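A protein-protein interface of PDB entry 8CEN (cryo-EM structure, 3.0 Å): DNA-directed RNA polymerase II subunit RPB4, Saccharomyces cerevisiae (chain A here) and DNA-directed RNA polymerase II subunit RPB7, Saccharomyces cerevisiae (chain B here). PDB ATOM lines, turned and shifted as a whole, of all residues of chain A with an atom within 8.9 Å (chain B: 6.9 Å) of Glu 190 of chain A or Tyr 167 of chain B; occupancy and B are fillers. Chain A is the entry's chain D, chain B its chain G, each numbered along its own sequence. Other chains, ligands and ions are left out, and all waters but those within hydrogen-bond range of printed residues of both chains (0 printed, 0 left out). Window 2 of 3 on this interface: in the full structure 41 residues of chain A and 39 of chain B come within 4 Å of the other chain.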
ATOM      1  N   LEU A 180      -4.869   3.788  15.630  1.00  0.00           N
ATOM      2  CA  LEU A 180      -4.802   2.374  15.262  1.00  0.00           C
ATOM      3  C   LEU A 180      -4.146   2.182  13.900  1.00  0.00           C
ATOM      4  O   LEU A 180      -3.362   1.245  13.708  1.00  0.00           O
ATOM      5  CB  LEU A 180      -6.201   1.759  15.269  1.00  0.00           C
ATOM      6  CG  LEU A 180      -6.850   1.520  16.633  1.00  0.00           C
ATOM      7  CD1 LEU A 180      -8.283   1.041  16.466  1.00  0.00           C
ATOM      8  CD2 LEU A 180      -6.038   0.518  17.433  1.00  0.00           C
ATOM      9  N   LEU A 183      -0.041   3.366  14.599  1.00  0.00           N
ATOM     10  CA  LEU A 183       0.823   2.512  15.404  1.00  0.00           C
ATOM     11  C   LEU A 183       0.827   1.088  14.861  1.00  0.00           C
ATOM     12  O   LEU A 183      -0.230   0.513  14.583  1.00  0.00           O
ATOM     13  CB  LEU A 183       0.365   2.520  16.861  1.00  0.00           C
ATOM     14  CG  LEU A 183       0.257   3.897  17.516  1.00  0.00           C
ATOM     15  CD1 LEU A 183      -0.220   3.771  18.955  1.00  0.00           C
ATOM     16  CD2 LEU A 183       1.586   4.627  17.445  1.00  0.00           C
ATOM     17  N   ALA A 184       2.023   0.518  14.715  1.00  0.00           N
ATOM     18  CA  ALA A 184       2.181  -0.848  14.215  1.00  0.00           C
ATOM     19  C   ALA A 184       2.077  -1.833  15.379  1.00  0.00           C
ATOM     20  O   ALA A 184       3.031  -2.516  15.759  1.00  0.00           O
ATOM     21  CB  ALA A 184       3.500  -0.992  13.469  1.00  0.00           C
ATOM     22  N   CYS A 185       0.879  -1.892  15.949  1.00  0.00           N
ATOM     23  CA  CYS A 185       0.622  -2.755  17.087  1.00  0.00           C
ATOM     24  C   CYS A 185       0.400  -4.197  16.638  1.00  0.00           C
ATOM     25  O   CYS A 185       0.160  -4.483  15.463  1.00  0.00           O
ATOM     26  CB  CYS A 185      -0.586  -2.259  17.875  1.00  0.00           C
ATOM     27  SG  CYS A 185      -0.792  -3.075  19.465  1.00  0.00           S
ATOM     28  N   ASP A 186       0.483  -5.110  17.602  1.00  0.00           N
ATOM     29  CA  ASP A 186       0.364  -6.536  17.327  1.00  0.00           C
ATOM     30  C   ASP A 186      -0.788  -7.184  18.082  1.00  0.00           C
ATOM     31  O   ASP A 186      -1.577  -7.914  17.477  1.00  0.00           O
ATOM     32  CB  ASP A 186       1.694  -7.235  17.689  1.00  0.00           C
ATOM     33  CG  ASP A 186       1.765  -8.697  17.234  1.00  0.00           C
ATOM     34  OD1 ASP A 186       0.799  -9.237  16.654  1.00  0.00           O
ATOM     35  OD2 ASP A 186       2.822  -9.320  17.477  1.00  0.00           O
ATOM     36  N   THR A 187      -0.927  -6.923  19.379  1.00  0.00           N
ATOM     37  CA  THR A 187      -1.913  -7.608  20.201  1.00  0.00           C
ATOM     38  C   THR A 187      -2.896  -6.616  20.810  1.00  0.00           C
ATOM     39  O   THR A 187      -2.648  -5.408  20.866  1.00  0.00           O
ATOM     40  CB  THR A 187      -1.249  -8.426  21.319  1.00  0.00           C
ATOM     41  OG1 THR A 187      -0.513  -7.554  22.183  1.00  0.00           O
ATOM     42  CG2 THR A 187      -0.306  -9.473  20.736  1.00  0.00           C
ATOM     43  N   ALA A 188      -4.026  -7.162  21.273  1.00  0.00           N
ATOM     44  CA  ALA A 188      -5.107  -6.336  21.804  1.00  0.00           C
ATOM     45  C   ALA A 188      -4.702  -5.627  23.090  1.00  0.00           C
ATOM     46  O   ALA A 188      -4.995  -4.440  23.261  1.00  0.00           O
ATOM     47  CB  ALA A 188      -6.352  -7.191  22.036  1.00  0.00           C
ATOM     48  N   ASP A 189      -4.037  -6.337  24.006  1.00  0.00           N
ATOM     49  CA  ASP A 189      -3.617  -5.728  25.266  1.00  0.00           C
ATOM     50  C   ASP A 189      -2.562  -4.652  25.018  1.00  0.00           C
ATOM     51  O   ASP A 189      -2.574  -3.603  25.676  1.00  0.00           O
ATOM     52  CB  ASP A 189      -3.090  -6.821  26.206  1.00  0.00           C
ATOM     53  CG  ASP A 189      -2.828  -6.333  27.636  1.00  0.00           C
ATOM     54  OD1 ASP A 189      -3.015  -5.140  27.953  1.00  0.00           O
ATOM     55  OD2 ASP A 189      -2.419  -7.176  28.463  1.00  0.00           O
ATOM     56  N   GLU A 190      -1.666  -4.887  24.055  1.00  0.00           N
ATOM     57  CA  GLU A 190      -0.698  -3.863  23.674  1.00  0.00           C
ATOM     58  C   GLU A 190      -1.395  -2.647  23.077  1.00  0.00           C
ATOM     59  O   GLU A 190      -0.983  -1.509  23.326  1.00  0.00           O
ATOM     60  CB  GLU A 190       0.322  -4.439  22.693  1.00  0.00           C
ATOM     61  CG  GLU A 190       1.429  -3.474  22.303  1.00  0.00           C
ATOM     62  CD  GLU A 190       2.555  -4.154  21.551  1.00  0.00           C
ATOM     63  OE1 GLU A 190       3.492  -4.653  22.207  1.00  0.00           O
ATOM     64  OE2 GLU A 190       2.501  -4.188  20.304  1.00  0.00           O
ATOM     65  N   ALA A 191      -2.463  -2.866  22.304  1.00  0.00           N
ATOM     66  CA  ALA A 191      -3.243  -1.746  21.783  1.00  0.00           C
ATOM     67  C   ALA A 191      -3.913  -0.961  22.905  1.00  0.00           C
ATOM     68  O   ALA A 191      -3.937   0.275  22.877  1.00  0.00           O
ATOM     69  CB  ALA A 191      -4.284  -2.249  20.783  1.00  0.00           C
ATOM     70  N   LYS A 192      -4.462  -1.665  23.901  1.00  0.00           N
ATOM     71  CA  LYS A 192      -5.112  -0.993  25.025  1.00  0.00           C
ATOM     72  C   LYS A 192      -4.118  -0.182  25.848  1.00  0.00           C
ATOM     73  O   LYS A 192      -4.440   0.920  26.305  1.00  0.00           O
ATOM     74  CB  LYS A 192      -5.832  -2.006  25.921  1.00  0.00           C
ATOM     75  CG  LYS A 192      -6.888  -2.855  25.230  1.00  0.00           C
ATOM     76  CD  LYS A 192      -8.146  -2.075  24.891  1.00  0.00           C
ATOM     77  CE  LYS A 192      -9.134  -2.102  26.045  1.00  0.00           C
ATOM     78  NZ  LYS A 192     -10.495  -1.679  25.615  1.00  0.00           N
ATOM     79  N   THR A 193      -2.909  -0.707  26.061  1.00  0.00           N
ATOM     80  CA  THR A 193      -1.940   0.052  26.844  1.00  0.00           C
ATOM     81  C   THR A 193      -1.240   1.136  26.027  1.00  0.00           C
ATOM     82  O   THR A 193      -0.729   2.094  26.615  1.00  0.00           O
ATOM     83  CB  THR A 193      -0.902  -0.876  27.491  1.00  0.00           C
ATOM     84  OG1 THR A 193      -0.077  -0.118  28.384  1.00  0.00           O
ATOM     85  CG2 THR A 193      -0.018  -1.534  26.452  1.00  0.00           C
ATOM     86  N   LEU A 194      -1.207   1.016  24.696  1.00  0.00           N
ATOM     87  CA  LEU A 194      -0.693   2.102  23.871  1.00  0.00           C
ATOM     88  C   LEU A 194      -1.696   3.243  23.770  1.00  0.00           C
ATOM     89  O   LEU A 194      -1.316   4.416  23.851  1.00  0.00           O
ATOM     90  CB  LEU A 194      -0.337   1.586  22.475  1.00  0.00           C
ATOM     91  CG  LEU A 194       1.050   0.972  22.283  1.00  0.00           C
ATOM     92  CD1 LEU A 194       1.361   0.809  20.804  1.00  0.00           C
ATOM     93  CD2 LEU A 194       2.113   1.819  22.958  1.00  0.00           C
ATOM     94  N   ILE A 195      -2.970   2.921  23.598  1.00  0.00           N
ATOM     95  CA  ILE A 195      -4.038   3.906  23.528  1.00  0.00           C
ATOM     96  C   ILE A 195      -4.967   3.677  24.712  1.00  0.00           C
ATOM     97  O   ILE A 195      -5.850   2.820  24.664  1.00  0.00           O
ATOM     98  CB  ILE A 195      -4.806   3.813  22.198  1.00  0.00           C
ATOM     99  CG1 ILE A 195      -3.839   3.634  21.025  1.00  0.00           C
ATOM    100  CG2 ILE A 195      -5.671   5.046  21.996  1.00  0.00           C
ATOM    101  CD1 ILE A 195      -4.501   3.142  19.760  1.00  0.00           C
ATOM    102  N   PRO A 196      -4.795   4.430  25.804  1.00  0.00           N
ATOM    103  CA  PRO A 196      -5.734   4.327  26.935  1.00  0.00           C
ATOM    104  C   PRO A 196      -7.143   4.784  26.597  1.00  0.00           C
ATOM    105  O   PRO A 196      -8.071   4.495  27.365  1.00  0.00           O
ATOM    106  CB  PRO A 196      -5.101   5.229  28.004  1.00  0.00           C
ATOM    107  CG  PRO A 196      -3.671   5.398  27.580  1.00  0.00           C
ATOM    108  CD  PRO A 196      -3.693   5.364  26.086  1.00  0.00           C
ATOM    109  N   LEU A 198      -8.914   3.558  24.300  1.00  0.00           N
ATOM    110  CA  LEU A 198      -9.658   2.389  23.850  1.00  0.00           C
ATOM    111  C   LEU A 198     -10.233   1.562  24.993  1.00  0.00           C
ATOM    112  O   LEU A 198     -10.862   0.531  24.724  1.00  0.00           O
ATOM    113  CB  LEU A 198      -8.765   1.499  22.982  1.00  0.00           C
ATOM    114  CG  LEU A 198      -8.428   2.017  21.586  1.00  0.00           C
ATOM    115  CD1 LEU A 198      -7.481   1.061  20.880  1.00  0.00           C
ATOM    116  CD2 LEU A 198      -9.694   2.216  20.774  1.00  0.00           C
ATOM    117  N   ASP A 204     -12.240  -7.372  23.137  1.00  0.00           N
ATOM    118  CA  ASP A 204     -10.888  -7.882  22.927  1.00  0.00           C
ATOM    119  C   ASP A 204     -10.784  -8.716  21.654  1.00  0.00           C
ATOM    120  O   ASP A 204      -9.794  -8.610  20.921  1.00  0.00           O
ATOM    121  CB  ASP A 204     -10.448  -8.699  24.141  1.00  0.00           C
ATOM    122  CG  ASP A 204     -10.182  -7.835  25.358  1.00  0.00           C
ATOM    123  OD1 ASP A 204     -10.076  -6.601  25.198  1.00  0.00           O
ATOM    124  OD2 ASP A 204     -10.083  -8.388  26.473  1.00  0.00           O
ATOM    125  N   LEU A 207     -10.925  -6.375  18.684  1.00  0.00           N
ATOM    126  CA  LEU A 207      -9.663  -5.649  18.591  1.00  0.00           C
ATOM    127  C   LEU A 207      -8.564  -6.526  18.001  1.00  0.00           C
ATOM    128  O   LEU A 207      -7.857  -6.112  17.074  1.00  0.00           O
ATOM    129  CB  LEU A 207      -9.254  -5.130  19.970  1.00  0.00           C
ATOM    130  CG  LEU A 207      -8.209  -4.012  19.983  1.00  0.00           C
ATOM    131  CD1 LEU A 207      -8.716  -2.790  19.234  1.00  0.00           C
ATOM    132  CD2 LEU A 207      -7.824  -3.653  21.408  1.00  0.00           C
ATOM    133  N   LEU A 211      -6.785  -5.755  14.317  1.00  0.00           N
ATOM    134  CA  LEU A 211      -5.332  -5.666  14.196  1.00  0.00           C
ATOM    135  C   LEU A 211      -4.720  -6.842  13.441  1.00  0.00           C
ATOM    136  O   LEU A 211      -3.647  -6.682  12.852  1.00  0.00           O
ATOM    137  CB  LEU A 211      -4.662  -5.507  15.565  1.00  0.00           C
ATOM    138  CG  LEU A 211      -4.647  -4.135  16.258  1.00  0.00           C
ATOM    139  CD1 LEU A 211      -5.962  -3.624  16.806  1.00  0.00           C
ATOM    140  CD2 LEU A 211      -3.631  -4.207  17.379  1.00  0.00           C
ATOM    141  N   VAL B  86       0.846   8.228  21.886  1.00  0.00           N
ATOM    142  CA  VAL B  86       1.979   7.399  21.488  1.00  0.00           C
ATOM    143  C   VAL B  86       2.258   7.631  20.009  1.00  0.00           C
ATOM    144  O   VAL B  86       1.374   7.439  19.165  1.00  0.00           O
ATOM    145  CB  VAL B  86       1.710   5.915  21.777  1.00  0.00           C
ATOM    146  CG1 VAL B  86       2.767   5.051  21.126  1.00  0.00           C
ATOM    147  CG2 VAL B  86       1.682   5.675  23.275  1.00  0.00           C
ATOM    148  N   ARG B 144       9.600   4.072  19.491  1.00  0.00           N
ATOM    149  CA  ARG B 144       8.225   4.443  19.796  1.00  0.00           C
ATOM    150  C   ARG B 144       8.179   5.086  21.175  1.00  0.00           C
ATOM    151  O   ARG B 144       8.707   4.523  22.140  1.00  0.00           O
ATOM    152  CB  ARG B 144       7.322   3.210  19.743  1.00  0.00           C
ATOM    153  CG  ARG B 144       5.925   3.425  20.271  1.00  0.00           C
ATOM    154  CD  ARG B 144       5.192   2.101  20.412  1.00  0.00           C
ATOM    155  NE  ARG B 144       5.422   1.231  19.265  1.00  0.00           N
ATOM    156  CZ  ARG B 144       4.637   1.176  18.198  1.00  0.00           C
ATOM    157  NH1 ARG B 144       3.553   1.927  18.099  1.00  0.00           N
ATOM    158  NH2 ARG B 144       4.947   0.347  17.205  1.00  0.00           N
ATOM    159  N   ILE B 163       9.512   6.568  27.706  1.00  0.00           N
ATOM    160  CA  ILE B 163       9.411   5.193  27.228  1.00  0.00           C
ATOM    161  C   ILE B 163       9.424   4.244  28.420  1.00  0.00           C
ATOM    162  O   ILE B 163       9.726   3.053  28.275  1.00  0.00           O
ATOM    163  CB  ILE B 163      10.545   4.854  26.243  1.00  0.00           C
ATOM    164  CG1 ILE B 163      11.907   5.149  26.875  1.00  0.00           C
ATOM    165  CG2 ILE B 163      10.378   5.621  24.934  1.00  0.00           C
ATOM    166  CD1 ILE B 163      13.073   4.587  26.094  1.00  0.00           C
ATOM    167  N   LYS B 164       9.090   4.761  29.605  1.00  0.00           N
ATOM    168  CA  LYS B 164       9.088   3.934  30.807  1.00  0.00           C
ATOM    169  C   LYS B 164       7.905   2.977  30.848  1.00  0.00           C
ATOM    170  O   LYS B 164       7.940   2.001  31.604  1.00  0.00           O
ATOM    171  CB  LYS B 164       9.098   4.814  32.057  1.00  0.00           C
ATOM    172  CG  LYS B 164      10.459   5.418  32.354  1.00  0.00           C
ATOM    173  CD  LYS B 164      10.558   5.920  33.783  1.00  0.00           C
ATOM    174  CE  LYS B 164      10.457   4.773  34.775  1.00  0.00           C
ATOM    175  NZ  LYS B 164      10.845   5.205  36.144  1.00  0.00           N
ATOM    176  N   GLU B 165       6.858   3.244  30.074  1.00  0.00           N
ATOM    177  CA  GLU B 165       5.764   2.294  29.941  1.00  0.00           C
ATOM    178  C   GLU B 165       6.222   1.062  29.168  1.00  0.00           C
ATOM    179  O   GLU B 165       7.087   1.135  28.291  1.00  0.00           O
ATOM    180  CB  GLU B 165       4.573   2.939  29.230  1.00  0.00           C
ATOM    181  CG  GLU B 165       3.884   4.067  29.992  1.00  0.00           C
ATOM    182  CD  GLU B 165       3.186   3.593  31.252  1.00  0.00           C
ATOM    183  OE1 GLU B 165       2.704   2.440  31.273  1.00  0.00           O
ATOM    184  OE2 GLU B 165       3.102   4.381  32.215  1.00  0.00           O
ATOM    185  N   ASP B 166       5.636  -0.082  29.516  1.00  0.00           N
ATOM    186  CA  ASP B 166       5.929  -1.321  28.812  1.00  0.00           C
ATOM    187  C   ASP B 166       5.402  -1.267  27.382  1.00  0.00           C
ATOM    188  O   ASP B 166       4.461  -0.532  27.071  1.00  0.00           O
ATOM    189  CB  ASP B 166       5.323  -2.516  29.550  1.00  0.00           C
ATOM    190  CG  ASP B 166       6.228  -3.040  30.648  1.00  0.00           C
ATOM    191  OD1 ASP B 166       7.441  -3.191  30.394  1.00  0.00           O
ATOM    192  OD2 ASP B 166       5.727  -3.305  31.762  1.00  0.00           O
ATOM    193  N   TYR B 167       6.045  -2.055  26.511  1.00  0.00           N
ATOM    194  CA  TYR B 167       5.748  -2.134  25.074  1.00  0.00           C
ATOM    195  C   TYR B 167       5.950  -0.791  24.377  1.00  0.00           C
ATOM    196  O   TYR B 167       5.238  -0.455  23.427  1.00  0.00           O
ATOM    197  CB  TYR B 167       4.340  -2.689  24.803  1.00  0.00           C
ATOM    198  CG  TYR B 167       4.039  -4.032  25.449  1.00  0.00           C
ATOM    199  CD1 TYR B 167       5.060  -4.922  25.783  1.00  0.00           C
ATOM    200  CD2 TYR B 167       2.733  -4.400  25.744  1.00  0.00           C
ATOM    201  CE1 TYR B 167       4.785  -6.137  26.377  1.00  0.00           C
ATOM    202  CE2 TYR B 167       2.449  -5.615  26.340  1.00  0.00           C
ATOM    203  CZ  TYR B 167       3.480  -6.479  26.654  1.00  0.00           C
ATOM    204  OH  TYR B 167       3.206  -7.690  27.246  1.00  0.00           O
ATOM    205  N   LEU B 168       6.923  -0.020  24.849  1.00  0.00           N
ATOM    206  CA  LEU B 168       7.423   1.178  24.187  1.00  0.00           C
ATOM    207  C   LEU B 168       8.913   1.004  23.903  1.00  0.00           C
ATOM    208  O   LEU B 168       9.484  -0.074  24.095  1.00  0.00           O
ATOM    209  CB  LEU B 168       7.162   2.430  25.029  1.00  0.00           C
ATOM    210  CG  LEU B 168       5.814   3.141  24.900  1.00  0.00           C
ATOM    211  CD1 LEU B 168       4.697   2.378  25.582  1.00  0.00           C
ATOM    212  CD2 LEU B 168       5.920   4.546  25.460  1.00  0.00           C
ATOM    213  N   GLY B 169       9.544   2.078  23.441  1.00  0.00           N
ATOM    214  CA  GLY B 169      10.969   2.051  23.185  1.00  0.00           C
ATOM    215  C   GLY B 169      11.311   1.782  21.736  1.00  0.00           C
ATOM    216  O   GLY B 169      10.567   2.180  20.834  1.00  0.00           O
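Glu 190 of chain A touches just one residue of chain B: Tyr 167 (3.3 Å). Of the printed residues of chain B, Leu 194 of chain A touches Val 86, Arg 144, Tyr 167 and Leu 168. Of the printed residues of chain B, Ala 184 of chain A touches Arg 144 (3.7 Å). Of the printed residues of chain A, Leu 168 of chain B touches Leu 194. Of the printed residues of chain B, Leu 183 of chain A touches Val 86 (3.3 Å) and Arg 144 (3.4 Å). Ile 195 of chain A touches none of the printed residues of chain B. The nearest residue of chain B that does not touch Glu 190 of chain A is Arg 144 of chain B (6.0 Å). The nearest residue of chain A that does not touch Tyr 167 of chain B is Thr 193 of chain A (4.04 Å).
The backbone NH (N) of Glu 190 of chain A sits close to the side-chain hydroxyl (OG1) of Thr 187 of chain A, at 3.5 Å. The backbone carbonyl oxygen (O) of Gly 169 of chain B lies within hydrogen-bond range of the backbone NH (N) of Arg 144 of chain B (2.5 Å). The backbone NH (N) of Asp 186 of chain A is in hydrogen-bond range of the side-chain carboxylate (OE2) of Glu 190 of chain A, at 3.5 Å. The side-chain sulfur of Cys 185 of chain A lies within hydrogen-bond range of the side-chain carboxylate of Glu 190 of chain A, 3.6 Å away.
Of the 9 printed residues of chain B, 4 touch a printed residue of chain A. Hydrophobic or aromatic side chains of chain B that line the printed part of chain A: Val 86, Tyr 167 and Leu 168. Of the 19 printed residues of chain A, 4 touch a printed residue of chain B. Hydrophobic or aromatic side chains of chain A within 4 Å of the printed part of chain B: Leu 183 and Leu 194.
Among the printed residues, merely in contact across the chains: Leu 194 of chain A with Val 86 of chain B (3.3 Å), Leu 183 of chain A with Val 86 of chain B (3.3 Å), Glu 190 of chain A with Tyr 167 of chain B (3.3 Å), Leu 183 of chain A with Arg 144 of chain B (3.4 Å), Leu 194 of chain A with Arg 144 of chain B (3.7 Å), Leu 194 of chain A with Leu 168 of chain B (3.7 Å), Ala 184 of chain A with Arg 144 of chain B (3.7 Å) and Leu 194 of chain A with Tyr 167 of chain B (3.9 Å).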
